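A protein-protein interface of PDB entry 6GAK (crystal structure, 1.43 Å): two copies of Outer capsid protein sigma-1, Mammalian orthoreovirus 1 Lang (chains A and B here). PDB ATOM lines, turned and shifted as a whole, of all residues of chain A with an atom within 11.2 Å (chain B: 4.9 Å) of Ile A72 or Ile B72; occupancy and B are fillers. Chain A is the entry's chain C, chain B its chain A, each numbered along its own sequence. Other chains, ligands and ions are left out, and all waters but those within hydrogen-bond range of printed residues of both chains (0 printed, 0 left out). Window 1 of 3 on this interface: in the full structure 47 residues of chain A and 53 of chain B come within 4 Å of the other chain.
Asn A68 touches its own counterpart, Asn B68.
Asn A68 touches Thr B69, but with the chains exchanged Thr A69 does not touch Asn B68 (7.9 Å).
Ser A71 touches Ile B72, but with the chains exchanged Ile A72 does not touch Ser B71 (7.7 Å).
Leu A75 touches Gly B76, but with the chains exchanged Gly A76 does not touch Leu B75 (8.0 Å).
Positions printed for both chains: 68, 69, 70, 71, 72, 73, 74, 75 and 76.
Asn B68 touches Asn A68.
Ile B72 touches Asn A68.
CB of Ser A71 touches CG2 of Ile B72 (3.7 Å).
CG1 of Ile A72 touches CD1 of Ile B72, at 3.8 Å.
Ile B72 touches Leu A75 (O to CD1, 3.8 Å).
Leu B75 touches Leu A75.
Leu A75 touches Gly B76 (CD2 to CA, 3.9 Å).
Hydrophobic or aromatic side chains of chain A that line the printed part of chain B: Ile A72 and Leu A75.
Printed residues of chain B that touch a printed residue of chain A: Asn B68, Thr B69, Ile B72, Leu B75 and Gly B76.
Hydrophobic or aromatic side chains of chain B that line the printed part of chain A: Ile B72 and Leu B75.
Among the printed residues, no Asp or Glu carboxylate lies within 4 Å of a Lys or Arg side-chain nitrogen of the other chain.
Of the printed residues of chain B, Asn A68 touches Asn B68, Thr B69 and Ile B72.
Of the printed residues of chain B, Ser A71 touches Ile B72 (3.7 Å).
Ile A72 touches one residue of chain B.
Printed residues of chain B within 4 Å of Leu A75: Ile B72 (3.8 Å), Leu B75 (3.9 Å) and Gly B76 (3.9 Å).
Asp A77 touches none of the printed residues of chain B.
Ala A81 touches none of the printed residues of chain B.
Asn B68 touches just one residue of chain A: Asn A68.
Thr B69 touches one residue of chain A.
Ser B71 touches none of the printed residues of chain A.
Of chain A, only Asn A68, Ser A71, Ile A72 and Leu A75 come within 4 Å of Ile B72.
Gly B76 touches one residue of chain A.
The nearest printed residue of chain B that does not touch Ile A72 is Asn B68 (6.0 Å).
The nearest residue of chain A that does not touch Ile B72 is Thr A69 (5.5 Å).
The backbone carbonyl oxygen (O) of Gln A67 sits at hydrogen-bond distance from the side-chain hydroxyl (OG) of Ser A71, 3.1 Å away.
The side-chain hydroxyl (OG1) of Thr B69 lies within hydrogen-bond range of the side-chain amide nitrogen (ND2) of Asn A68.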
ATOM      1  N   LEU A  61     -25.329 -24.589   9.877  1.00  0.00           N
ATOM      2  CA  LEU A  61     -26.035 -24.971  11.093  1.00  0.00           C
ATOM      3  C   LEU A  61     -25.039 -25.176  12.242  1.00  0.00           C
ATOM      4  O   LEU A  61     -25.312 -24.724  13.375  1.00  0.00           O
ATOM      5  CB  LEU A  61     -26.878 -26.217  10.833  1.00  0.00           C
ATOM      6  CG  LEU A  61     -27.996 -26.497  11.846  1.00  0.00           C
ATOM      7  CD1 LEU A  61     -28.907 -25.225  12.080  1.00  0.00           C
ATOM      8  CD2 LEU A  61     -28.807 -27.691  11.385  1.00  0.00           C
ATOM      9  N   ASN A  63     -22.174 -23.704  12.662  1.00  0.00           N
ATOM     10  CA  ASN A  63     -21.700 -22.392  13.072  1.00  0.00           C
ATOM     11  C   ASN A  63     -22.776 -21.718  13.932  1.00  0.00           C
ATOM     12  O   ASN A  63     -22.382 -21.152  14.964  1.00  0.00           O
ATOM     13  CB  ASN A  63     -21.214 -21.562  11.860  1.00  0.00           C
ATOM     14  CG  ASN A  63     -20.508 -20.259  12.241  1.00  0.00           C
ATOM     15  OD1 ASN A  63     -19.480 -20.248  12.935  1.00  0.00           O
ATOM     16  ND2 ASN A  63     -21.045 -19.132  11.796  1.00  0.00           N
ATOM     17  N   SER A  64     -24.094 -21.827  13.589  1.00  0.00           N
ATOM     18  CA  SER A  64     -25.136 -21.232  14.419  1.00  0.00           C
ATOM     19  C   SER A  64     -25.218 -21.900  15.783  1.00  0.00           C
ATOM     20  O   SER A  64     -25.416 -21.182  16.776  1.00  0.00           O
ATOM     21  CB  SER A  64     -26.494 -21.241  13.736  1.00  0.00           C
ATOM     22  OG  SER A  64     -26.944 -22.574  13.587  1.00  0.00           O
ATOM     23  N   VAL A  65     -25.009 -23.241  15.840  1.00  0.00           N
ATOM     24  CA  VAL A  65     -25.033 -23.973  17.112  1.00  0.00           C
ATOM     25  C   VAL A  65     -23.841 -23.544  17.961  1.00  0.00           C
ATOM     26  O   VAL A  65     -24.027 -23.309  19.164  1.00  0.00           O
ATOM     27  CB  VAL A  65     -25.041 -25.509  16.852  1.00  0.00           C
ATOM     28  CG1 VAL A  65     -24.872 -26.289  18.179  1.00  0.00           C
ATOM     29  CG2 VAL A  65     -26.335 -25.899  16.151  1.00  0.00           C
ATOM     30  N   SER A  66     -22.655 -23.364  17.357  1.00  0.00           N
ATOM     31  CA  SER A  66     -21.427 -22.923  18.023  1.00  0.00           C
ATOM     32  C   SER A  66     -21.642 -21.532  18.616  1.00  0.00           C
ATOM     33  O   SER A  66     -21.274 -21.304  19.793  1.00  0.00           O
ATOM     34  CB  SER A  66     -20.262 -22.917  17.039  1.00  0.00           C
ATOM     35  OG  SER A  66     -19.059 -22.561  17.704  1.00  0.00           O
ATOM     36  N   GLN A  67     -22.330 -20.653  17.873  1.00  0.00           N
ATOM     37  CA  GLN A  67     -22.652 -19.297  18.355  1.00  0.00           C
ATOM     38  C   GLN A  67     -23.588 -19.388  19.542  1.00  0.00           C
ATOM     39  O   GLN A  67     -23.374 -18.665  20.545  1.00  0.00           O
ATOM     40  CB  GLN A  67     -23.237 -18.448  17.248  1.00  0.00           C
ATOM     41  CG  GLN A  67     -22.137 -18.128  16.212  1.00  0.00           C
ATOM     42  CD  GLN A  67     -22.612 -17.426  14.975  1.00  0.00           C
ATOM     43  OE1 GLN A  67     -23.691 -17.695  14.460  1.00  0.00           O
ATOM     44  NE2 GLN A  67     -21.775 -16.538  14.444  1.00  0.00           N
ATOM     45  N   ASN A  68     -24.571 -20.300  19.494  1.00  0.00           N
ATOM     46  CA  ASN A  68     -25.507 -20.500  20.615  1.00  0.00           C
ATOM     47  C   ASN A  68     -24.765 -21.062  21.822  1.00  0.00           C
ATOM     48  O   ASN A  68     -25.039 -20.610  22.932  1.00  0.00           O
ATOM     49  CB  ASN A  68     -26.695 -21.377  20.244  1.00  0.00           C
ATOM     50  CG  ASN A  68     -27.714 -20.658  19.348  1.00  0.00           C
ATOM     51  OD1 ASN A  68     -27.649 -19.431  19.151  1.00  0.00           O
ATOM     52  ND2 ASN A  68     -28.719 -21.437  18.840  1.00  0.00           N
ATOM     53  N   THR A  69     -23.837 -22.041  21.654  1.00  0.00           N
ATOM     54  CA  THR A  69     -23.067 -22.571  22.790  1.00  0.00           C
ATOM     55  C   THR A  69     -22.282 -21.426  23.449  1.00  0.00           C
ATOM     56  O   THR A  69     -22.265 -21.312  24.684  1.00  0.00           O
ATOM     57  CB  THR A  69     -22.111 -23.656  22.304  1.00  0.00           C
ATOM     58  OG1 THR A  69     -22.899 -24.643  21.661  1.00  0.00           O
ATOM     59  CG2 THR A  69     -21.329 -24.288  23.440  1.00  0.00           C
ATOM     60  N   GLN A  70     -21.693 -20.524  22.654  1.00  0.00           N
ATOM     61  CA  GLN A  70     -20.940 -19.362  23.185  1.00  0.00           C
ATOM     62  C   GLN A  70     -21.904 -18.396  23.923  1.00  0.00           C
ATOM     63  O   GLN A  70     -21.581 -17.958  25.043  1.00  0.00           O
ATOM     64  CB  GLN A  70     -20.274 -18.602  22.031  1.00  0.00           C
ATOM     65  CG  GLN A  70     -19.305 -17.517  22.522  1.00  0.00           C
ATOM     66  N   SER A  71     -23.086 -18.107  23.364  1.00  0.00           N
ATOM     67  CA  SER A  71     -24.068 -17.234  24.019  1.00  0.00           C
ATOM     68  C   SER A  71     -24.536 -17.847  25.341  1.00  0.00           C
ATOM     69  O   SER A  71     -24.685 -17.121  26.342  1.00  0.00           O
ATOM     70  CB  SER A  71     -25.281 -17.029  23.141  1.00  0.00           C
ATOM     71  OG  SER A  71     -24.960 -16.347  21.933  1.00  0.00           O
ATOM     72  N   ILE A  72     -24.766 -19.166  25.385  1.00  0.00           N
ATOM     73  CA  ILE A  72     -25.196 -19.851  26.600  1.00  0.00           C
ATOM     74  C   ILE A  72     -24.097 -19.733  27.665  1.00  0.00           C
ATOM     75  O   ILE A  72     -24.415 -19.471  28.846  1.00  0.00           O
ATOM     76  CB  ILE A  72     -25.511 -21.331  26.265  1.00  0.00           C
ATOM     77  CG1 ILE A  72     -26.842 -21.413  25.567  1.00  0.00           C
ATOM     78  CG2 ILE A  72     -25.496 -22.236  27.539  1.00  0.00           C
ATOM     79  CD1 ILE A  72     -27.023 -22.732  24.750  1.00  0.00           C
ATOM     80  N   SER A  73     -22.821 -19.910  27.278  1.00  0.00           N
ATOM     81  CA  SER A  73     -21.681 -19.810  28.211  1.00  0.00           C
ATOM     82  C   SER A  73     -21.626 -18.380  28.807  1.00  0.00           C
ATOM     83  O   SER A  73     -21.448 -18.228  30.037  1.00  0.00           O
ATOM     84  CB  SER A  73     -20.401 -20.092  27.439  1.00  0.00           C
ATOM     85  OG  SER A  73     -19.283 -20.042  28.297  1.00  0.00           O
ATOM     86  N   SER A  74     -21.822 -17.343  27.956  1.00  0.00           N
ATOM     87  CA  SER A  74     -21.847 -15.948  28.372  1.00  0.00           C
ATOM     88  C   SER A  74     -23.014 -15.688  29.364  1.00  0.00           C
ATOM     89  O   SER A  74     -22.819 -15.039  30.419  1.00  0.00           O
ATOM     90  CB  SER A  74     -21.931 -15.037  27.155  1.00  0.00           C
ATOM     91  OG  SER A  74     -22.012 -13.677  27.555  1.00  0.00           O
ATOM     92  N   LEU A  75     -24.208 -16.188  29.065  1.00  0.00           N
ATOM     93  CA  LEU A  75     -25.351 -15.994  29.972  1.00  0.00           C
ATOM     94  C   LEU A  75     -25.063 -16.734  31.291  1.00  0.00           C
ATOM     95  O   LEU A  75     -25.404 -16.184  32.351  1.00  0.00           O
ATOM     96  CB  LEU A  75     -26.641 -16.520  29.357  1.00  0.00           C
ATOM     97  CG  LEU A  75     -27.176 -15.754  28.146  1.00  0.00           C
ATOM     98  CD1 LEU A  75     -28.393 -16.491  27.494  1.00  0.00           C
ATOM     99  CD2 LEU A  75     -27.473 -14.301  28.500  1.00  0.00           C
ATOM    100  N   GLY A  76     -24.435 -17.907  31.247  1.00  0.00           N
ATOM    101  CA  GLY A  76     -24.055 -18.665  32.444  1.00  0.00           C
ATOM    102  C   GLY A  76     -23.108 -17.864  33.320  1.00  0.00           C
ATOM    103  O   GLY A  76     -23.315 -17.756  34.535  1.00  0.00           O
ATOM    104  N   ASP A  77     -22.151 -17.183  32.693  1.00  0.00           N
ATOM    105  CA  ASP A  77     -21.183 -16.329  33.438  1.00  0.00           C
ATOM    106  C   ASP A  77     -21.931 -15.187  34.131  1.00  0.00           C
ATOM    107  O   ASP A  77     -21.676 -14.880  35.299  1.00  0.00           O
ATOM    108  CB  ASP A  77     -20.159 -15.732  32.473  1.00  0.00           C
ATOM    109  CG  ASP A  77     -19.076 -16.706  32.006  1.00  0.00           C
ATOM    110  OD1 ASP A  77     -18.948 -17.794  32.609  1.00  0.00           O
ATOM    111  OD2 ASP A  77     -18.407 -16.402  30.981  1.00  0.00           O
ATOM    112  N   ARG A  78     -22.919 -14.605  33.457  1.00  0.00           N
ATOM    113  CA  ARG A  78     -23.678 -13.469  33.995  1.00  0.00           C
ATOM    114  C   ARG A  78     -24.579 -13.926  35.184  1.00  0.00           C
ATOM    115  O   ARG A  78     -24.627 -13.232  36.207  1.00  0.00           O
ATOM    116  CB  ARG A  78     -24.463 -12.768  32.913  1.00  0.00           C
ATOM    117  CG  ARG A  78     -23.539 -12.051  31.910  1.00  0.00           C
ATOM    118  CD  ARG A  78     -24.276 -11.567  30.664  1.00  0.00           C
ATOM    119  NE  ARG A  78     -25.205 -10.479  30.944  1.00  0.00           N
ATOM    120  CZ  ARG A  78     -26.110 -10.002  30.092  1.00  0.00           C
ATOM    121  NH1 ARG A  78     -26.262 -10.552  28.891  1.00  0.00           N
ATOM    122  NH2 ARG A  78     -26.928  -9.030  30.464  1.00  0.00           N
ATOM    123  N   ILE A  79     -25.250 -15.083  35.068  1.00  0.00           N
ATOM    124  CA  ILE A  79     -26.071 -15.592  36.168  1.00  0.00           C
ATOM    125  C   ILE A  79     -25.151 -16.056  37.325  1.00  0.00           C
ATOM    126  O   ILE A  79     -25.500 -15.844  38.484  1.00  0.00           O
ATOM    127  CB  ILE A  79     -27.039 -16.701  35.680  1.00  0.00           C
ATOM    128  CG1 ILE A  79     -28.054 -16.134  34.632  1.00  0.00           C
ATOM    129  CG2 ILE A  79     -27.709 -17.462  36.825  1.00  0.00           C
ATOM    130  CD1 ILE A  79     -28.709 -17.243  33.836  1.00  0.00           C
ATOM    131  N   ASN A  80     -23.966 -16.600  37.029  1.00  0.00           N
ATOM    132  CA  ASN A  80     -23.010 -17.027  38.060  1.00  0.00           C
ATOM    133  C   ASN A  80     -22.618 -15.790  38.871  1.00  0.00           C
ATOM    134  O   ASN A  80     -22.352 -15.912  40.062  1.00  0.00           O
ATOM    135  CB  ASN A  80     -21.732 -17.576  37.404  1.00  0.00           C
ATOM    136  CG  ASN A  80     -21.788 -19.031  37.007  1.00  0.00           C
ATOM    137  OD1 ASN A  80     -22.717 -19.731  37.308  1.00  0.00           O
ATOM    138  ND2 ASN A  80     -20.779 -19.502  36.318  1.00  0.00           N
ATOM    139  N   ALA A  81     -22.459 -14.647  38.193  1.00  0.00           N
ATOM    140  CA  ALA A  81     -22.037 -13.426  38.894  1.00  0.00           C
ATOM    141  C   ALA A  81     -23.184 -12.830  39.699  1.00  0.00           C
ATOM    142  O   ALA A  81     -22.941 -12.309  40.813  1.00  0.00           O
ATOM    143  CB  ALA A  81     -21.515 -12.411  37.887  1.00  0.00           C
ATOM    144  N   ASN B  68     -33.798 -22.437  19.905  1.00  0.00           N
ATOM    145  CA  ASN B  68     -32.747 -22.147  20.900  1.00  0.00           C
ATOM    146  C   ASN B  68     -32.238 -20.719  20.775  1.00  0.00           C
ATOM    147  O   ASN B  68     -32.098 -20.045  21.777  1.00  0.00           O
ATOM    148  CB  ASN B  68     -31.578 -23.150  20.806  1.00  0.00           C
ATOM    149  CG  ASN B  68     -31.954 -24.538  21.344  1.00  0.00           C
ATOM    150  OD1 ASN B  68     -32.994 -24.734  22.015  1.00  0.00           O
ATOM    151  ND2 ASN B  68     -31.072 -25.502  21.149  1.00  0.00           N
ATOM    152  N   THR B  69     -31.966 -20.231  19.528  1.00  0.00           N
ATOM    153  CA  THR B  69     -31.522 -18.848  19.369  1.00  0.00           C
ATOM    154  C   THR B  69     -32.556 -17.867  19.961  1.00  0.00           C
ATOM    155  O   THR B  69     -32.146 -16.909  20.660  1.00  0.00           O
ATOM    156  CB  THR B  69     -31.365 -18.559  17.870  1.00  0.00           C
ATOM    157  OG1 THR B  69     -30.475 -19.500  17.338  1.00  0.00           O
ATOM    158  CG2 THR B  69     -30.744 -17.174  17.608  1.00  0.00           C
ATOM    159  N   GLN B  70     -33.881 -18.143  19.755  1.00  0.00           N
ATOM    160  CA  GLN B  70     -34.966 -17.318  20.275  1.00  0.00           C
ATOM    161  C   GLN B  70     -34.985 -17.358  21.813  1.00  0.00           C
ATOM    162  O   GLN B  70     -35.120 -16.308  22.482  1.00  0.00           O
ATOM    163  CB  GLN B  70     -36.325 -17.783  19.732  1.00  0.00           C
ATOM    164  CG  GLN B  70     -36.677 -17.177  18.385  1.00  0.00           C
ATOM    165  CD  GLN B  70     -37.747 -17.930  17.622  1.00  0.00           C
ATOM    166  OE1 GLN B  70     -37.556 -18.296  16.445  1.00  0.00           O
ATOM    167  NE2 GLN B  70     -38.879 -18.205  18.267  1.00  0.00           N
ATOM    168  N   SER B  71     -34.874 -18.575  22.384  1.00  0.00           N
ATOM    169  CA  SER B  71     -34.880 -18.742  23.856  1.00  0.00           C
ATOM    170  C   SER B  71     -33.679 -17.994  24.459  1.00  0.00           C
ATOM    171  O   SER B  71     -33.813 -17.395  25.535  1.00  0.00           O
ATOM    172  CB  SER B  71     -34.713 -20.221  24.189  1.00  0.00           C
ATOM    173  OG  SER B  71     -35.853 -20.981  23.841  1.00  0.00           O
ATOM    174  N   ILE B  72     -32.509 -18.043  23.806  1.00  0.00           N
ATOM    175  CA  ILE B  72     -31.303 -17.365  24.272  1.00  0.00           C
ATOM    176  C   ILE B  72     -31.538 -15.829  24.284  1.00  0.00           C
ATOM    177  O   ILE B  72     -31.178 -15.159  25.248  1.00  0.00           O
ATOM    178  CB  ILE B  72     -30.080 -17.767  23.442  1.00  0.00           C
ATOM    179  CG1 ILE B  72     -29.632 -19.177  23.848  1.00  0.00           C
ATOM    180  CG2 ILE B  72     -28.912 -16.774  23.566  1.00  0.00           C
ATOM    181  CD1 ILE B  72     -28.754 -19.830  22.714  1.00  0.00           C
ATOM    182  N   SER B  73     -32.198 -15.302  23.259  1.00  0.00           N
ATOM    183  CA  SER B  73     -32.493 -13.853  23.198  1.00  0.00           C
ATOM    184  C   SER B  73     -33.454 -13.487  24.367  1.00  0.00           C
ATOM    185  O   SER B  73     -33.271 -12.449  25.022  1.00  0.00           O
ATOM    186  CB  SER B  73     -33.156 -13.574  21.850  1.00  0.00           C
ATOM    187  OG  SER B  73     -33.623 -12.234  21.777  1.00  0.00           O
ATOM    188  N   SER B  74     -34.461 -14.339  24.658  1.00  0.00           N
ATOM    189  CA  SER B  74     -35.415 -14.091  25.756  1.00  0.00           C
ATOM    190  C   SER B  74     -34.657 -14.108  27.120  1.00  0.00           C
ATOM    191  O   SER B  74     -34.908 -13.244  27.975  1.00  0.00           O
ATOM    192  CB  SER B  74     -36.496 -15.155  25.784  1.00  0.00           C
ATOM    193  OG  SER B  74     -37.499 -14.868  26.741  1.00  0.00           O
ATOM    194  N   LEU B  75     -33.746 -15.090  27.309  1.00  0.00           N
ATOM    195  CA  LEU B  75     -32.996 -15.128  28.573  1.00  0.00           C
ATOM    196  C   LEU B  75     -32.108 -13.893  28.685  1.00  0.00           C
ATOM    197  O   LEU B  75     -31.989 -13.346  29.789  1.00  0.00           O
ATOM    198  CB  LEU B  75     -32.135 -16.392  28.607  1.00  0.00           C
ATOM    199  CG  LEU B  75     -32.918 -17.713  28.773  1.00  0.00           C
ATOM    200  CD1 LEU B  75     -31.979 -18.862  28.757  1.00  0.00           C
ATOM    201  CD2 LEU B  75     -33.866 -17.708  30.009  1.00  0.00           C
ATOM    202  N   GLY B  76     -31.500 -13.451  27.568  1.00  0.00           N
ATOM    203  CA  GLY B  76     -30.664 -12.251  27.507  1.00  0.00           C
ATOM    204  C   GLY B  76     -31.457 -11.024  27.954  1.00  0.00           C
ATOM    205  O   GLY B  76     -30.977 -10.252  28.795  1.00  0.00           O
